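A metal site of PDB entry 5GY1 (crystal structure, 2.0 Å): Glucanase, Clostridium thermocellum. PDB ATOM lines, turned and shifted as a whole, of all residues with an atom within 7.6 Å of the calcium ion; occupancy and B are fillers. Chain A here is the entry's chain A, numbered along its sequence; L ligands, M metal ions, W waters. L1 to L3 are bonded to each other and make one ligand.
The indole nitrogen (NE1) of Trp 245 is in hydrogen-bond range of an oxygen (O3) of LIG L1 (2.9 Å).
The side-chain carboxylate (OD2) of Asp 246 lies within hydrogen-bond range of an oxygen (O1) of LG3 L3.
SG of Cys 244 sits at hydrogen-bond distance from O5 of LG2 L2 (3.4 Å).
O2 of LG3 L3 is in hydrogen-bond range of OD2 of Asp 247 (3.3 Å).
The side-chain carboxylate (OD2) of Asp 199 sits close to the backbone NH (N) of Cys 248 (3.5 Å).
OD1 of Asp 246 sits at hydrogen-bond distance from N of His 194.
ND2 of Asn 229 sits at hydrogen-bond distance from O of Ser 195, 2.9 Å away.
The backbone NH (N) of Asp 246 sits close to the side-chain sulfur (SG) of Cys 244 (3.7 Å).
Within 4 Å of the calcium ion: Ser 195, Gly 196, Asp 199, Glu 200 and Asp 246.
The nearest printed residue that does not touch the calcium ion is Asp 247 (4.3 Å).
The calcium ion is bound by the backbone carbonyl oxygen (O) of Asp 246 (2.3 Å), the backbone carbonyl oxygen (O) of Gly 196 (2.3 Å), water W1 (2.4 Å), the side-chain carboxylate (OE2) of Glu 200 (2.5 Å), the side-chain hydroxyl (OG) of Ser 195 (2.5 Å), the side-chain carboxylate (OD2) of Asp 199 (2.6 Å), the side-chain carboxylate (OE1) of Glu 200 (2.6 Å) and the side-chain carboxylate (OD1) of Asp 199 (2.6 Å).
Water W1 bridges OD1 of Asp 246 and OG of Ser 193.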
ATOM      1  N   LEU A  59       9.639 -32.969  13.537  1.00  0.00           N
ATOM      2  CA  LEU A  59      10.988 -32.483  13.229  1.00  0.00           C
ATOM      3  C   LEU A  59      11.835 -33.558  12.534  1.00  0.00           C
ATOM      4  O   LEU A  59      12.278 -33.352  11.395  1.00  0.00           O
ATOM      5  CB  LEU A  59      11.655 -31.843  14.475  1.00  0.00           C
ATOM      6  CG  LEU A  59      13.072 -31.256  14.341  1.00  0.00           C
ATOM      7  CD1 LEU A  59      13.154 -30.227  13.198  1.00  0.00           C
ATOM      8  CD2 LEU A  59      13.570 -30.642  15.635  1.00  0.00           C
ATOM      9  N   ALA A 143      11.953 -24.052  14.268  1.00  0.00           N
ATOM     10  CA  ALA A 143      12.742 -25.197  13.800  1.00  0.00           C
ATOM     11  C   ALA A 143      11.860 -26.251  13.130  1.00  0.00           C
ATOM     12  O   ALA A 143      12.109 -26.714  12.001  1.00  0.00           O
ATOM     13  CB  ALA A 143      13.517 -25.811  14.976  1.00  0.00           C
ATOM     14  N   VAL A 144      10.787 -26.631  13.805  1.00  0.00           N
ATOM     15  CA  VAL A 144       9.943 -27.684  13.236  1.00  0.00           C
ATOM     16  C   VAL A 144       9.190 -27.207  11.996  1.00  0.00           C
ATOM     17  O   VAL A 144       9.108 -27.913  10.987  1.00  0.00           O
ATOM     18  CB  VAL A 144       9.000 -28.353  14.265  1.00  0.00           C
ATOM     19  CG1 VAL A 144       7.906 -27.404  14.733  1.00  0.00           C
ATOM     20  CG2 VAL A 144       8.397 -29.635  13.653  1.00  0.00           C
ATOM     21  N   GLN A 147      11.731 -26.899   9.160  1.00  0.00           N
ATOM     22  CA  GLN A 147      12.065 -28.212   8.581  1.00  0.00           C
ATOM     23  C   GLN A 147      10.961 -28.747   7.681  1.00  0.00           C
ATOM     24  O   GLN A 147      11.244 -29.248   6.582  1.00  0.00           O
ATOM     25  CB  GLN A 147      12.467 -29.247   9.641  1.00  0.00           C
ATOM     26  CG  GLN A 147      13.072 -30.567   9.086  1.00  0.00           C
ATOM     27  CD  GLN A 147      14.373 -30.376   8.320  1.00  0.00           C
ATOM     28  OE1 GLN A 147      14.458 -30.661   7.123  1.00  0.00           O
ATOM     29  NE2 GLN A 147      15.415 -29.901   9.018  1.00  0.00           N
ATOM     30  N   ASP A 181      11.362 -20.926  19.091  1.00  0.00           N
ATOM     31  CA  ASP A 181      11.004 -22.310  19.400  1.00  0.00           C
ATOM     32  C   ASP A 181      10.133 -22.465  20.644  1.00  0.00           C
ATOM     33  O   ASP A 181       9.920 -23.580  21.123  1.00  0.00           O
ATOM     34  CB  ASP A 181      12.269 -23.158  19.547  1.00  0.00           C
ATOM     35  CG  ASP A 181      12.885 -23.524  18.197  1.00  0.00           C
ATOM     36  OD1 ASP A 181      12.115 -23.718  17.230  1.00  0.00           O
ATOM     37  OD2 ASP A 181      14.115 -23.687  18.111  1.00  0.00           O
ATOM     38  N   SER A 192      14.127 -32.421  21.460  1.00  0.00           N
ATOM     39  CA  SER A 192      14.270 -31.013  21.848  1.00  0.00           C
ATOM     40  C   SER A 192      15.076 -30.255  20.799  1.00  0.00           C
ATOM     41  O   SER A 192      15.967 -30.806  20.188  1.00  0.00           O
ATOM     42  CB  SER A 192      15.031 -30.899  23.173  1.00  0.00           C
ATOM     43  OG  SER A 192      14.225 -31.415  24.218  1.00  0.00           O
ATOM     44  N   SER A 193      14.778 -28.972  20.627  1.00  0.00           N
ATOM     45  CA  SER A 193      15.569 -28.178  19.698  1.00  0.00           C
ATOM     46  C   SER A 193      16.838 -27.796  20.457  1.00  0.00           C
ATOM     47  O   SER A 193      16.775 -27.021  21.406  1.00  0.00           O
ATOM     48  CB  SER A 193      14.777 -26.941  19.278  1.00  0.00           C
ATOM     49  OG  SER A 193      15.534 -26.122  18.410  1.00  0.00           O
ATOM     50  N   HIS A 194      17.976 -28.351  20.069  1.00  0.00           N
ATOM     51  CA  HIS A 194      19.228 -28.110  20.794  1.00  0.00           C
ATOM     52  C   HIS A 194      19.979 -26.916  20.185  1.00  0.00           C
ATOM     53  O   HIS A 194      20.401 -26.002  20.875  1.00  0.00           O
ATOM     54  CB  HIS A 194      20.090 -29.380  20.785  1.00  0.00           C
ATOM     55  CG  HIS A 194      19.475 -30.535  21.506  1.00  0.00           C
ATOM     56  ND1 HIS A 194      19.760 -30.844  22.823  1.00  0.00           N
ATOM     57  CD2 HIS A 194      18.578 -31.466  21.089  1.00  0.00           C
ATOM     58  CE1 HIS A 194      19.062 -31.907  23.186  1.00  0.00           C
ATOM     59  NE2 HIS A 194      18.341 -32.305  22.155  1.00  0.00           N
ATOM     60  N   SER A 195      20.092 -26.914  18.856  1.00  0.00           N
ATOM     61  CA  SER A 195      20.828 -25.880  18.153  1.00  0.00           C
ATOM     62  C   SER A 195      20.075 -24.555  17.976  1.00  0.00           C
ATOM     63  O   SER A 195      20.679 -23.569  17.570  1.00  0.00           O
ATOM     64  CB  SER A 195      21.268 -26.411  16.776  1.00  0.00           C
ATOM     65  OG  SER A 195      20.153 -26.962  16.065  1.00  0.00           O
ATOM     66  N   GLY A 196      18.772 -24.523  18.248  1.00  0.00           N
ATOM     67  CA  GLY A 196      17.966 -23.359  17.885  1.00  0.00           C
ATOM     68  C   GLY A 196      17.439 -23.491  16.464  1.00  0.00           C
ATOM     69  O   GLY A 196      17.570 -24.538  15.819  1.00  0.00           O
ATOM     70  N   PHE A 197      16.842 -22.405  15.952  1.00  0.00           N
ATOM     71  CA  PHE A 197      16.077 -22.482  14.708  1.00  0.00           C
ATOM     72  C   PHE A 197      16.742 -21.813  13.505  1.00  0.00           C
ATOM     73  O   PHE A 197      16.239 -21.929  12.384  1.00  0.00           O
ATOM     74  CB  PHE A 197      14.686 -21.874  14.914  1.00  0.00           C
ATOM     75  CG  PHE A 197      14.736 -20.434  15.331  1.00  0.00           C
ATOM     76  CD1 PHE A 197      14.997 -19.435  14.400  1.00  0.00           C
ATOM     77  CD2 PHE A 197      14.603 -20.086  16.669  1.00  0.00           C
ATOM     78  CE1 PHE A 197      15.096 -18.090  14.796  1.00  0.00           C
ATOM     79  CE2 PHE A 197      14.693 -18.753  17.074  1.00  0.00           C
ATOM     80  CZ  PHE A 197      14.934 -17.755  16.122  1.00  0.00           C
ATOM     81  N   TRP A 198      17.875 -21.128  13.709  1.00  0.00           N
ATOM     82  CA  TRP A 198      18.471 -20.377  12.606  1.00  0.00           C
ATOM     83  C   TRP A 198      18.962 -21.322  11.519  1.00  0.00           C
ATOM     84  O   TRP A 198      18.904 -20.997  10.326  1.00  0.00           O
ATOM     85  CB  TRP A 198      19.587 -19.428  13.057  1.00  0.00           C
ATOM     86  CG  TRP A 198      19.136 -18.335  13.988  1.00  0.00           C
ATOM     87  CD1 TRP A 198      19.357 -18.258  15.334  1.00  0.00           C
ATOM     88  CD2 TRP A 198      18.369 -17.168  13.647  1.00  0.00           C
ATOM     89  NE1 TRP A 198      18.770 -17.126  15.845  1.00  0.00           N
ATOM     90  CE2 TRP A 198      18.166 -16.441  14.833  1.00  0.00           C
ATOM     91  CE3 TRP A 198      17.825 -16.683  12.441  1.00  0.00           C
ATOM     92  CZ2 TRP A 198      17.440 -15.239  14.863  1.00  0.00           C
ATOM     93  CZ3 TRP A 198      17.119 -15.480  12.471  1.00  0.00           C
ATOM     94  CH2 TRP A 198      16.928 -14.773  13.677  1.00  0.00           C
ATOM     95  N   ASP A 199      19.420 -22.517  11.905  1.00  0.00           N
ATOM     96  CA  ASP A 199      19.820 -23.471  10.867  1.00  0.00           C
ATOM     97  C   ASP A 199      18.643 -23.974  10.026  1.00  0.00           C
ATOM     98  O   ASP A 199      18.802 -24.192   8.822  1.00  0.00           O
ATOM     99  CB  ASP A 199      20.614 -24.642  11.449  1.00  0.00           C
ATOM    100  CG  ASP A 199      19.879 -25.305  12.582  1.00  0.00           C
ATOM    101  OD1 ASP A 199      19.809 -24.715  13.676  1.00  0.00           O
ATOM    102  OD2 ASP A 199      19.324 -26.402  12.375  1.00  0.00           O
ATOM    103  N   GLU A 200      17.486 -24.179  10.634  1.00  0.00           N
ATOM    104  CA  GLU A 200      16.310 -24.593   9.856  1.00  0.00           C
ATOM    105  C   GLU A 200      15.839 -23.487   8.917  1.00  0.00           C
ATOM    106  O   GLU A 200      15.381 -23.780   7.812  1.00  0.00           O
ATOM    107  CB  GLU A 200      15.129 -25.048  10.738  1.00  0.00           C
ATOM    108  CG  GLU A 200      15.307 -26.423  11.376  1.00  0.00           C
ATOM    109  CD  GLU A 200      16.115 -26.385  12.679  1.00  0.00           C
ATOM    110  OE1 GLU A 200      16.516 -25.286  13.083  1.00  0.00           O
ATOM    111  OE2 GLU A 200      16.375 -27.432  13.316  1.00  0.00           O
ATOM    112  N   LEU A 201      15.914 -22.225   9.340  1.00  0.00           N
ATOM    113  CA  LEU A 201      15.546 -21.140   8.422  1.00  0.00           C
ATOM    114  C   LEU A 201      16.535 -21.097   7.257  1.00  0.00           C
ATOM    115  O   LEU A 201      16.141 -20.843   6.117  1.00  0.00           O
ATOM    116  CB  LEU A 201      15.518 -19.785   9.136  1.00  0.00           C
ATOM    117  CG  LEU A 201      14.469 -19.601  10.246  1.00  0.00           C
ATOM    118  CD1 LEU A 201      14.456 -18.148  10.743  1.00  0.00           C
ATOM    119  CD2 LEU A 201      13.074 -19.969   9.716  1.00  0.00           C
ATOM    120  N   ASN A 229      25.314 -20.974  15.242  1.00  0.00           N
ATOM    121  CA  ASN A 229      26.163 -21.150  16.411  1.00  0.00           C
ATOM    122  C   ASN A 229      27.621 -21.215  16.001  1.00  0.00           C
ATOM    123  O   ASN A 229      27.920 -21.675  14.903  1.00  0.00           O
ATOM    124  CB  ASN A 229      25.767 -22.418  17.173  1.00  0.00           C
ATOM    125  CG  ASN A 229      24.312 -22.392  17.573  1.00  0.00           C
ATOM    126  OD1 ASN A 229      23.846 -21.391  18.092  1.00  0.00           O
ATOM    127  ND2 ASN A 229      23.576 -23.452  17.265  1.00  0.00           N
ATOM    128  N   CYS A 244      21.965 -33.453  10.724  1.00  0.00           N
ATOM    129  CA  CYS A 244      21.023 -34.315  11.429  1.00  0.00           C
ATOM    130  C   CYS A 244      19.686 -33.632  11.647  1.00  0.00           C
ATOM    131  O   CYS A 244      19.519 -32.444  11.344  1.00  0.00           O
ATOM    132  CB  CYS A 244      21.598 -34.730  12.787  1.00  0.00           C
ATOM    133  SG  CYS A 244      21.781 -33.346  13.946  1.00  0.00           S
ATOM    134  N   TRP A 245      18.757 -34.379  12.234  1.00  0.00           N
ATOM    135  CA  TRP A 245      17.387 -33.899  12.416  1.00  0.00           C
ATOM    136  C   TRP A 245      17.309 -32.548  13.150  1.00  0.00           C
ATOM    137  O   TRP A 245      16.355 -31.802  12.945  1.00  0.00           O
ATOM    138  CB  TRP A 245      16.552 -34.954  13.178  1.00  0.00           C
ATOM    139  CG  TRP A 245      17.107 -35.261  14.569  1.00  0.00           C
ATOM    140  CD1 TRP A 245      17.903 -36.305  14.924  1.00  0.00           C
ATOM    141  CD2 TRP A 245      16.871 -34.507  15.765  1.00  0.00           C
ATOM    142  NE1 TRP A 245      18.197 -36.252  16.280  1.00  0.00           N
ATOM    143  CE2 TRP A 245      17.571 -35.154  16.819  1.00  0.00           C
ATOM    144  CE3 TRP A 245      16.125 -33.353  16.063  1.00  0.00           C
ATOM    145  CZ2 TRP A 245      17.559 -34.685  18.131  1.00  0.00           C
ATOM    146  CZ3 TRP A 245      16.122 -32.883  17.376  1.00  0.00           C
ATOM    147  CH2 TRP A 245      16.825 -33.550  18.390  1.00  0.00           C
ATOM    148  N   ASP A 246      18.294 -32.263  13.992  1.00  0.00           N
ATOM    149  CA  ASP A 246      18.326 -31.035  14.804  1.00  0.00           C
ATOM    150  C   ASP A 246      19.030 -29.863  14.124  1.00  0.00           C
ATOM    151  O   ASP A 246      18.804 -28.706  14.480  1.00  0.00           O
ATOM    152  CB  ASP A 246      19.018 -31.299  16.148  1.00  0.00           C
ATOM    153  CG  ASP A 246      18.968 -30.080  17.069  1.00  0.00           C
ATOM    154  OD1 ASP A 246      17.847 -29.725  17.471  1.00  0.00           O
ATOM    155  OD2 ASP A 246      20.016 -29.485  17.369  1.00  0.00           O
ATOM    156  N   ASP A 247      19.856 -30.169  13.128  1.00  0.00           N
ATOM    157  CA  ASP A 247      20.802 -29.172  12.627  1.00  0.00           C
ATOM    158  C   ASP A 247      21.258 -29.530  11.214  1.00  0.00           C
ATOM    159  O   ASP A 247      22.016 -30.473  10.991  1.00  0.00           O
ATOM    160  CB  ASP A 247      21.980 -29.053  13.587  1.00  0.00           C
ATOM    161  CG  ASP A 247      22.855 -27.846  13.301  1.00  0.00           C
ATOM    162  OD1 ASP A 247      22.664 -27.165  12.265  1.00  0.00           O
ATOM    163  OD2 ASP A 247      23.752 -27.578  14.121  1.00  0.00           O
ATOM    164  N   CYS A 248      20.737 -28.769  10.265  1.00  0.00           N
ATOM    165  CA  CYS A 248      20.973 -29.015   8.842  1.00  0.00           C
ATOM    166  C   CYS A 248      21.835 -27.942   8.201  1.00  0.00           C
ATOM    167  O   CYS A 248      21.869 -27.859   6.973  1.00  0.00           O
ATOM    168  CB  CYS A 248      19.626 -29.084   8.100  1.00  0.00           C
ATOM    169  SG  CYS A 248      18.752 -30.640   8.327  1.00  0.00           S
ATOM    170  N   HIS A 249      22.493 -27.111   9.012  1.00  0.00           N
ATOM    171  CA  HIS A 249      23.316 -26.052   8.401  1.00  0.00           C
ATOM    172  C   HIS A 249      24.499 -26.583   7.625  1.00  0.00           C
ATOM    173  O   HIS A 249      24.912 -25.942   6.667  1.00  0.00           O
ATOM    174  CB  HIS A 249      23.706 -24.947   9.375  1.00  0.00           C
ATOM    175  CG  HIS A 249      24.863 -25.260  10.265  1.00  0.00           C
ATOM    176  ND1 HIS A 249      24.719 -25.924  11.466  1.00  0.00           N
ATOM    177  CD2 HIS A 249      26.171 -24.934  10.172  1.00  0.00           C
ATOM    178  CE1 HIS A 249      25.893 -26.038  12.051  1.00  0.00           C
ATOM    179  NE2 HIS A 249      26.787 -25.431  11.299  1.00  0.00           N
HETATM  180  C1  LIG L   1      18.185 -39.233  19.085  1.00  0.00           C
HETATM  181  C2  LIG L   1      19.455 -38.416  19.345  1.00  0.00           C
HETATM  182  C3  LIG L   1      19.232 -37.450  20.507  1.00  0.00           C
HETATM  183  C4  LIG L   1      18.616 -38.115  21.751  1.00  0.00           C
HETATM  184  C5  LIG L   1      18.059 -37.083  22.740  1.00  0.00           C
HETATM  185  C6  LIG L   1      17.730 -39.926  20.382  1.00  0.00           C
HETATM  186  O1  LIG L   1      16.488 -40.621  20.196  1.00  0.00           O
HETATM  187  O2  LIG L   1      18.488 -40.227  18.094  1.00  0.00           O
HETATM  188  O3  LIG L   1      19.849 -37.741  18.137  1.00  0.00           O
HETATM  189  O4  LIG L   1      20.469 -36.850  20.890  1.00  0.00           O
HETATM  190  O5  LIG L   1      17.506 -38.904  21.345  1.00  0.00           O
HETATM  191  O6  LIG L   1      17.254 -36.111  22.042  1.00  0.00           O
HETATM  192  C1  LG2 L   2      21.732 -34.959  21.497  1.00  0.00           C
HETATM  193  C2  LG2 L   2      21.963 -33.495  21.168  1.00  0.00           C
HETATM  194  C3  LG2 L   2      22.169 -33.261  19.676  1.00  0.00           C
HETATM  195  C4  LG2 L   2      20.989 -33.866  18.913  1.00  0.00           C
HETATM  196  C5  LG2 L   2      21.226 -33.869  17.406  1.00  0.00           C
HETATM  197  C6  LG2 L   2      20.532 -35.434  20.677  1.00  0.00           C
HETATM  198  O1  LG2 L   2      21.348 -34.965  22.872  1.00  0.00           O
HETATM  199  O2  LG2 L   2      23.028 -32.950  21.937  1.00  0.00           O
HETATM  200  O3  LG2 L   2      22.211 -31.847  19.512  1.00  0.00           O
HETATM  201  O4  LG2 L   2      20.788 -35.228  19.295  1.00  0.00           O
HETATM  202  O5  LG2 L   2      22.454 -34.538  17.036  1.00  0.00           O
HETATM  203  C1  LG3 L   3      23.268 -30.097  18.152  1.00  0.00           C
HETATM  204  C2  LG3 L   3      24.618 -29.489  17.767  1.00  0.00           C
HETATM  205  C3  LG3 L   3      25.578 -29.445  18.943  1.00  0.00           C
HETATM  206  C4  LG3 L   3      25.626 -30.831  19.578  1.00  0.00           C
HETATM  207  C5  LG3 L   3      26.626 -30.903  20.732  1.00  0.00           C
HETATM  208  C6  LG3 L   3      23.439 -31.416  18.911  1.00  0.00           C
HETATM  209  O1  LG3 L   3      22.502 -30.295  16.965  1.00  0.00           O
HETATM  210  O2  LG3 L   3      24.392 -28.171  17.267  1.00  0.00           O
HETATM  211  O3  LG3 L   3      26.858 -29.060  18.421  1.00  0.00           O
HETATM  212  O4  LG3 L   3      24.316 -31.206  20.010  1.00  0.00           O
HETATM  213  O5  LG3 L   3      26.027 -30.351  21.907  1.00  0.00           O
HETATM  214 CA    CA M   1      18.177 -26.476  14.678  1.00  0.00          CA
HETATM  215  O   HOH W   1      17.022 -27.425  16.567  1.00  0.00           O
